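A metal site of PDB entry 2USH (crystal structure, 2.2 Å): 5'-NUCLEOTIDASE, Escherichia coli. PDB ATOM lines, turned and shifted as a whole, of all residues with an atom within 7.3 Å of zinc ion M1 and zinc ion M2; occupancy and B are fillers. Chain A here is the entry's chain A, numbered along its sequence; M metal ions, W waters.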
ATOM      1  N   ASN A  40     -31.871   4.062 -27.836  1.00  0.00           N
ATOM      2  CA  ASN A  40     -30.817   3.181 -27.336  1.00  0.00           C
ATOM      3  C   ASN A  40     -29.973   2.651 -28.469  1.00  0.00           C
ATOM      4  O   ASN A  40     -30.390   2.692 -29.615  1.00  0.00           O
ATOM      5  CB  ASN A  40     -31.413   1.978 -26.593  1.00  0.00           C
ATOM      6  CG  ASN A  40     -32.404   1.235 -27.438  1.00  0.00           C
ATOM      7  OD1 ASN A  40     -33.554   1.682 -27.614  1.00  0.00           O
ATOM      8  ND2 ASN A  40     -31.973   0.107 -27.993  1.00  0.00           N
ATOM      9  N   ASP A  41     -28.779   2.171 -28.139  1.00  0.00           N
ATOM     10  CA  ASP A  41     -27.897   1.566 -29.129  1.00  0.00           C
ATOM     11  C   ASP A  41     -27.710   2.381 -30.399  1.00  0.00           C
ATOM     12  O   ASP A  41     -27.882   1.887 -31.518  1.00  0.00           O
ATOM     13  CB  ASP A  41     -28.452   0.194 -29.420  1.00  0.00           C
ATOM     14  CG  ASP A  41     -28.519  -0.628 -28.162  1.00  0.00           C
ATOM     15  OD1 ASP A  41     -29.537  -0.572 -27.432  1.00  0.00           O
ATOM     16  OD2 ASP A  41     -27.499  -1.285 -27.887  1.00  0.00           O
ATOM     17  N   HIS A  42     -27.355   3.638 -30.158  1.00  0.00           N
ATOM     18  CA  HIS A  42     -27.063   4.667 -31.141  1.00  0.00           C
ATOM     19  C   HIS A  42     -25.915   4.205 -32.036  1.00  0.00           C
ATOM     20  O   HIS A  42     -25.955   4.371 -33.249  1.00  0.00           O
ATOM     21  CB  HIS A  42     -26.689   5.962 -30.403  1.00  0.00           C
ATOM     22  CG  HIS A  42     -26.291   7.078 -31.322  1.00  0.00           C
ATOM     23  ND1 HIS A  42     -27.183   7.669 -32.179  1.00  0.00           N
ATOM     24  CD2 HIS A  42     -25.083   7.631 -31.565  1.00  0.00           C
ATOM     25  CE1 HIS A  42     -26.540   8.550 -32.931  1.00  0.00           C
ATOM     26  NE2 HIS A  42     -25.263   8.541 -32.583  1.00  0.00           N
ATOM     27  N   HIS A  43     -24.889   3.636 -31.410  1.00  0.00           N
ATOM     28  CA  HIS A  43     -23.740   3.107 -32.128  1.00  0.00           C
ATOM     29  C   HIS A  43     -23.058   3.888 -33.269  1.00  0.00           C
ATOM     30  O   HIS A  43     -22.833   3.348 -34.335  1.00  0.00           O
ATOM     31  CB  HIS A  43     -24.049   1.670 -32.604  1.00  0.00           C
ATOM     32  CG  HIS A  43     -24.125   0.667 -31.486  1.00  0.00           C
ATOM     33  ND1 HIS A  43     -23.108   0.501 -30.571  1.00  0.00           N
ATOM     34  CD2 HIS A  43     -25.066  -0.246 -31.164  1.00  0.00           C
ATOM     35  CE1 HIS A  43     -23.413  -0.469 -29.739  1.00  0.00           C
ATOM     36  NE2 HIS A  43     -24.605  -0.939 -30.066  1.00  0.00           N
ATOM     37  N   GLY A  82     -30.818   4.351 -23.546  1.00  0.00           N
ATOM     38  CA  GLY A  82     -30.484   3.037 -23.013  1.00  0.00           C
ATOM     39  C   GLY A  82     -29.017   2.636 -23.223  1.00  0.00           C
ATOM     40  O   GLY A  82     -28.670   1.456 -23.044  1.00  0.00           O
ATOM     41  N   GLY A  83     -28.149   3.567 -23.630  1.00  0.00           N
ATOM     42  CA  GLY A  83     -26.744   3.221 -23.790  1.00  0.00           C
ATOM     43  C   GLY A  83     -26.253   2.747 -25.151  1.00  0.00           C
ATOM     44  O   GLY A  83     -27.043   2.631 -26.089  1.00  0.00           O
ATOM     45  N   ASP A  84     -24.974   2.373 -25.221  1.00  0.00           N
ATOM     46  CA  ASP A  84     -24.299   1.989 -26.478  1.00  0.00           C
ATOM     47  C   ASP A  84     -24.295   3.101 -27.532  1.00  0.00           C
ATOM     48  O   ASP A  84     -24.891   2.991 -28.595  1.00  0.00           O
ATOM     49  CB  ASP A  84     -24.835   0.687 -27.073  1.00  0.00           C
ATOM     50  CG  ASP A  84     -24.214  -0.538 -26.439  1.00  0.00           C
ATOM     51  OD1 ASP A  84     -23.334  -0.375 -25.579  1.00  0.00           O
ATOM     52  OD2 ASP A  84     -24.565  -1.669 -26.817  1.00  0.00           O
ATOM     53  N   ILE A  85     -23.608   4.185 -27.195  1.00  0.00           N
ATOM     54  CA  ILE A  85     -23.475   5.333 -28.059  1.00  0.00           C
ATOM     55  C   ILE A  85     -22.242   5.030 -28.907  1.00  0.00           C
ATOM     56  O   ILE A  85     -22.171   5.385 -30.083  1.00  0.00           O
ATOM     57  CB  ILE A  85     -23.210   6.614 -27.209  1.00  0.00           C
ATOM     58  CG1 ILE A  85     -24.300   6.713 -26.141  1.00  0.00           C
ATOM     59  CG2 ILE A  85     -23.129   7.854 -28.094  1.00  0.00           C
ATOM     60  CD1 ILE A  85     -25.707   6.679 -26.672  1.00  0.00           C
ATOM     61  N   ASN A  86     -21.268   4.366 -28.282  1.00  0.00           N
ATOM     62  CA  ASN A  86     -20.006   3.953 -28.890  1.00  0.00           C
ATOM     63  C   ASN A  86     -20.085   2.757 -29.814  1.00  0.00           C
ATOM     64  O   ASN A  86     -20.903   1.856 -29.626  1.00  0.00           O
ATOM     65  CB  ASN A  86     -18.945   3.592 -27.815  1.00  0.00           C
ATOM     66  CG  ASN A  86     -18.359   4.808 -27.093  1.00  0.00           C
ATOM     67  OD1 ASN A  86     -17.384   5.386 -27.559  1.00  0.00           O
ATOM     68  ND2 ASN A  86     -18.906   5.175 -25.941  1.00  0.00           N
ATOM     69  N   THR A  87     -19.188   2.765 -30.801  1.00  0.00           N
ATOM     70  CA  THR A  87     -18.968   1.657 -31.741  1.00  0.00           C
ATOM     71  C   THR A  87     -20.025   1.360 -32.777  1.00  0.00           C
ATOM     72  O   THR A  87     -21.127   0.995 -32.439  1.00  0.00           O
ATOM     73  CB  THR A  87     -18.725   0.383 -30.951  1.00  0.00           C
ATOM     74  OG1 THR A  87     -17.653   0.621 -30.011  1.00  0.00           O
ATOM     75  CG2 THR A  87     -18.349  -0.773 -31.874  1.00  0.00           C
ATOM     76  N   GLY A 115     -23.758   1.474 -21.521  1.00  0.00           N
ATOM     77  CA  GLY A 115     -23.851   0.203 -22.224  1.00  0.00           C
ATOM     78  C   GLY A 115     -22.564  -0.610 -22.244  1.00  0.00           C
ATOM     79  O   GLY A 115     -21.506  -0.147 -21.832  1.00  0.00           O
ATOM     80  N   ASN A 116     -22.638  -1.847 -22.721  1.00  0.00           N
ATOM     81  CA  ASN A 116     -21.450  -2.658 -22.755  1.00  0.00           C
ATOM     82  C   ASN A 116     -20.399  -2.078 -23.713  1.00  0.00           C
ATOM     83  O   ASN A 116     -19.208  -2.199 -23.468  1.00  0.00           O
ATOM     84  CB  ASN A 116     -21.814  -4.119 -23.096  1.00  0.00           C
ATOM     85  CG  ASN A 116     -22.482  -4.255 -24.449  1.00  0.00           C
ATOM     86  OD1 ASN A 116     -23.462  -3.588 -24.744  1.00  0.00           O
ATOM     87  ND2 ASN A 116     -21.958  -5.154 -25.280  1.00  0.00           N
ATOM     88  N   HIS A 117     -20.829  -1.431 -24.790  1.00  0.00           N
ATOM     89  CA  HIS A 117     -19.856  -0.848 -25.723  1.00  0.00           C
ATOM     90  C   HIS A 117     -19.206   0.484 -25.309  1.00  0.00           C
ATOM     91  O   HIS A 117     -18.440   1.062 -26.095  1.00  0.00           O
ATOM     92  CB  HIS A 117     -20.419  -0.729 -27.158  1.00  0.00           C
ATOM     93  CG  HIS A 117     -20.558  -2.052 -27.850  1.00  0.00           C
ATOM     94  ND1 HIS A 117     -19.492  -2.681 -28.462  1.00  0.00           N
ATOM     95  CD2 HIS A 117     -21.605  -2.912 -27.953  1.00  0.00           C
ATOM     96  CE1 HIS A 117     -19.861  -3.874 -28.884  1.00  0.00           C
ATOM     97  NE2 HIS A 117     -21.134  -4.035 -28.595  1.00  0.00           N
ATOM     98  N   THR A 172     -25.557  -4.405 -18.226  1.00  0.00           N
ATOM     99  CA  THR A 172     -25.425  -5.864 -18.325  1.00  0.00           C
ATOM    100  C   THR A 172     -24.087  -6.340 -17.782  1.00  0.00           C
ATOM    101  O   THR A 172     -23.025  -5.778 -18.065  1.00  0.00           O
ATOM    102  CB  THR A 172     -25.575  -6.388 -19.796  1.00  0.00           C
ATOM    103  OG1 THR A 172     -25.449  -7.816 -19.787  1.00  0.00           O
ATOM    104  CG2 THR A 172     -24.521  -5.793 -20.711  1.00  0.00           C
ATOM    105  N   THR A 175     -20.911  -7.581 -19.961  1.00  0.00           N
ATOM    106  CA  THR A 175     -19.927  -6.679 -20.512  1.00  0.00           C
ATOM    107  C   THR A 175     -18.536  -7.241 -20.432  1.00  0.00           C
ATOM    108  O   THR A 175     -17.772  -7.034 -21.341  1.00  0.00           O
ATOM    109  CB  THR A 175     -20.011  -5.315 -19.826  1.00  0.00           C
ATOM    110  OG1 THR A 175     -21.295  -4.750 -20.132  1.00  0.00           O
ATOM    111  CG2 THR A 175     -18.879  -4.372 -20.314  1.00  0.00           C
ATOM    112  N   HIS A 217     -29.224  -1.281 -19.688  1.00  0.00           N
ATOM    113  CA  HIS A 217     -28.646  -1.802 -20.916  1.00  0.00           C
ATOM    114  C   HIS A 217     -28.463  -3.311 -20.677  1.00  0.00           C
ATOM    115  O   HIS A 217     -27.351  -3.804 -20.501  1.00  0.00           O
ATOM    116  CB  HIS A 217     -27.338  -1.111 -21.205  1.00  0.00           C
ATOM    117  CG  HIS A 217     -26.851  -1.399 -22.570  1.00  0.00           C
ATOM    118  ND1 HIS A 217     -27.278  -0.661 -23.651  1.00  0.00           N
ATOM    119  CD2 HIS A 217     -26.107  -2.413 -23.058  1.00  0.00           C
ATOM    120  CE1 HIS A 217     -26.823  -1.222 -24.755  1.00  0.00           C
ATOM    121  NE2 HIS A 217     -26.123  -2.293 -24.423  1.00  0.00           N
ATOM    122  N   MET A 218     -29.593  -4.031 -20.686  1.00  0.00           N
ATOM    123  CA  MET A 218     -29.608  -5.462 -20.357  1.00  0.00           C
ATOM    124  C   MET A 218     -30.255  -6.383 -21.400  1.00  0.00           C
ATOM    125  O   MET A 218     -29.897  -7.548 -21.482  1.00  0.00           O
ATOM    126  CB  MET A 218     -30.278  -5.612 -18.975  1.00  0.00           C
ATOM    127  CG  MET A 218     -29.528  -4.828 -17.851  1.00  0.00           C
ATOM    128  SD  MET A 218     -30.427  -4.674 -16.279  1.00  0.00           S
ATOM    129  CE  MET A 218     -31.229  -6.274 -16.118  1.00  0.00           C
ATOM    130  N   GLY A 251     -32.328  -1.509 -23.683  1.00  0.00           N
ATOM    131  CA  GLY A 251     -31.433  -1.543 -24.833  1.00  0.00           C
ATOM    132  C   GLY A 251     -30.653  -2.844 -24.893  1.00  0.00           C
ATOM    133  O   GLY A 251     -31.055  -3.854 -24.297  1.00  0.00           O
ATOM    134  N   HIS A 252     -29.566  -2.831 -25.645  1.00  0.00           N
ATOM    135  CA  HIS A 252     -28.654  -3.952 -25.759  1.00  0.00           C
ATOM    136  C   HIS A 252     -29.084  -5.056 -26.701  1.00  0.00           C
ATOM    137  O   HIS A 252     -28.328  -5.437 -27.593  1.00  0.00           O
ATOM    138  CB  HIS A 252     -28.356  -4.551 -24.374  1.00  0.00           C
ATOM    139  CG  HIS A 252     -27.283  -5.603 -24.397  1.00  0.00           C
ATOM    140  ND1 HIS A 252     -26.040  -5.370 -24.929  1.00  0.00           N
ATOM    141  CD2 HIS A 252     -27.272  -6.879 -23.950  1.00  0.00           C
ATOM    142  CE1 HIS A 252     -25.305  -6.458 -24.817  1.00  0.00           C
ATOM    143  NE2 HIS A 252     -26.023  -7.384 -24.232  1.00  0.00           N
ATOM    144  N   SER A 253     -30.266  -5.609 -26.477  1.00  0.00           N
ATOM    145  CA  SER A 253     -30.777  -6.636 -27.370  1.00  0.00           C
ATOM    146  C   SER A 253     -31.103  -5.985 -28.727  1.00  0.00           C
ATOM    147  O   SER A 253     -31.107  -6.653 -29.731  1.00  0.00           O
ATOM    148  CB  SER A 253     -32.016  -7.338 -26.779  1.00  0.00           C
ATOM    149  OG  SER A 253     -33.100  -6.462 -26.489  1.00  0.00           O
ATOM    150  N   GLN A 254     -31.381  -4.675 -28.735  1.00  0.00           N
ATOM    151  CA  GLN A 254     -31.689  -3.917 -29.938  1.00  0.00           C
ATOM    152  C   GLN A 254     -32.905  -4.336 -30.733  1.00  0.00           C
ATOM    153  O   GLN A 254     -32.836  -4.541 -31.940  1.00  0.00           O
ATOM    154  CB  GLN A 254     -30.458  -3.857 -30.847  1.00  0.00           C
ATOM    155  CG  GLN A 254     -29.298  -3.174 -30.138  1.00  0.00           C
ATOM    156  CD  GLN A 254     -28.031  -3.125 -30.969  1.00  0.00           C
ATOM    157  OE1 GLN A 254     -26.922  -3.161 -30.433  1.00  0.00           O
ATOM    158  NE2 GLN A 254     -28.192  -3.026 -32.289  1.00  0.00           N
ATOM    159  N   HIS A 289     -35.203  -0.262 -30.524  1.00  0.00           N
ATOM    160  CA  HIS A 289     -34.432  -0.878 -31.567  1.00  0.00           C
ATOM    161  C   HIS A 289     -32.960  -0.434 -31.611  1.00  0.00           C
ATOM    162  O   HIS A 289     -32.170  -0.855 -30.762  1.00  0.00           O
ATOM    163  CB  HIS A 289     -35.139  -0.583 -32.888  1.00  0.00           C
ATOM    164  CG  HIS A 289     -34.582  -1.321 -34.049  1.00  0.00           C
ATOM    165  ND1 HIS A 289     -34.021  -2.573 -33.932  1.00  0.00           N
ATOM    166  CD2 HIS A 289     -34.539  -1.009 -35.369  1.00  0.00           C
ATOM    167  CE1 HIS A 289     -33.659  -3.007 -35.132  1.00  0.00           C
ATOM    168  NE2 HIS A 289     -33.972  -2.075 -36.016  1.00  0.00           N
ATOM    169  N   GLU A 290     -32.554   0.407 -32.556  1.00  0.00           N
ATOM    170  CA  GLU A 290     -31.151   0.761 -32.591  1.00  0.00           C
ATOM    171  C   GLU A 290     -30.919   1.885 -33.591  1.00  0.00           C
ATOM    172  O   GLU A 290     -31.794   2.199 -34.383  1.00  0.00           O
ATOM    173  CB  GLU A 290     -30.333  -0.447 -33.091  1.00  0.00           C
ATOM    174  CG  GLU A 290     -30.650  -0.690 -34.581  1.00  0.00           C
ATOM    175  CD  GLU A 290     -30.179  -2.011 -35.126  1.00  0.00           C
ATOM    176  OE1 GLU A 290     -29.744  -2.874 -34.342  1.00  0.00           O
ATOM    177  OE2 GLU A 290     -30.272  -2.182 -36.352  1.00  0.00           O
ATOM    178  N   TRP A 291     -29.700   2.455 -33.523  1.00  0.00           N
ATOM    179  CA  TRP A 291     -29.193   3.475 -34.445  1.00  0.00           C
ATOM    180  C   TRP A 291     -29.934   4.792 -34.683  1.00  0.00           C
ATOM    181  O   TRP A 291     -29.710   5.441 -35.709  1.00  0.00           O
ATOM    182  CB  TRP A 291     -28.974   2.834 -35.827  1.00  0.00           C
ATOM    183  CG  TRP A 291     -28.066   1.619 -35.825  1.00  0.00           C
ATOM    184  CD1 TRP A 291     -27.365   1.101 -34.771  1.00  0.00           C
ATOM    185  CD2 TRP A 291     -27.811   0.748 -36.952  1.00  0.00           C
ATOM    186  NE1 TRP A 291     -26.690  -0.031 -35.165  1.00  0.00           N
ATOM    187  CE2 TRP A 291     -26.948  -0.268 -36.495  1.00  0.00           C
ATOM    188  CE3 TRP A 291     -28.228   0.735 -38.297  1.00  0.00           C
ATOM    189  CZ2 TRP A 291     -26.487  -1.307 -37.344  1.00  0.00           C
ATOM    190  CZ3 TRP A 291     -27.771  -0.289 -39.140  1.00  0.00           C
ATOM    191  CH2 TRP A 291     -26.902  -1.296 -38.651  1.00  0.00           C
ATOM    192  N   THR A 518     -21.802  -9.793 -31.258  1.00  0.00           N
ATOM    193  CA  THR A 518     -20.837  -8.937 -30.534  1.00  0.00           C
ATOM    194  C   THR A 518     -21.049  -7.456 -30.722  1.00  0.00           C
ATOM    195  O   THR A 518     -20.562  -6.663 -29.941  1.00  0.00           O
ATOM    196  CB  THR A 518     -19.396  -9.196 -30.952  1.00  0.00           C
ATOM    197  OG1 THR A 518     -19.245  -8.831 -32.341  1.00  0.00           O
ATOM    198  CG2 THR A 518     -19.045 -10.668 -30.771  1.00  0.00           C
ATOM    199  N   GLY A 519     -21.762  -7.072 -31.766  1.00  0.00           N
ATOM    200  CA  GLY A 519     -21.916  -5.655 -31.982  1.00  0.00           C
ATOM    201  C   GLY A 519     -20.666  -5.067 -32.645  1.00  0.00           C
ATOM    202  O   GLY A 519     -20.624  -3.865 -32.850  1.00  0.00           O
HETATM  203 ZN    ZN M   1     -25.783  -2.189 -28.725  1.00  0.00          ZN
HETATM  204 ZN    ZN M   2     -25.179  -3.552 -25.747  1.00  0.00          ZN
HETATM  205  O   HOH W   1     -25.499  -3.995 -27.809  1.00  0.00           O
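The backbone carbonyl oxygen (O) of His 217 sits at hydrogen-bond distance from the backbone NH (N) of Thr 172 (3.0 Å). The side-chain carboxylate of Asp 41 sits at hydrogen-bond distance from the backbone NH of His 252, at 2.9 Å. N of Asp 41 is in hydrogen-bond range of O of Gly 83 (2.7 Å). OD1 of Asp 41 sits at hydrogen-bond distance from ND2 of Asn 40, 2.6 Å away. N of Trp 291 is in hydrogen-bond range of O of Asp 41, 2.8 Å away. OD1 of Asp 84 lies within hydrogen-bond range of N of His 117, 2.8 Å away. The backbone carbonyl oxygen of Asp 84 is in hydrogen-bond range of the backbone NH of His 42, 3.0 Å away. The side-chain amide nitrogen of Gln 254 is in hydrogen-bond range of the side-chain carboxylate of Glu 290 (2.6 Å).
Within 4 Å of zinc ion M1: Asp 41, His 43, Asp 84 and Gln 254. The nearest printed residue that does not touch zinc ion M1 is His 217 (4.2 Å).
The nearest printed residue that does not touch zinc ion M2 is His 117 (4.2 Å).
Zinc ion M1 is bound by water W1, the side-chain carboxylate (OD2) of Asp 41, a ring nitrogen (NE2) of His 43, the side-chain amide oxygen (OE1) of Gln 254 and the side-chain carboxylate (OD2) of Asp 84. Zinc ion M1 has five donor atoms within binding distance.
Zinc ion M2 is bound by OD1 of Asn 116, NE2 of His 217, water W1, ND1 of His 252 and OD2 of Asp 84.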
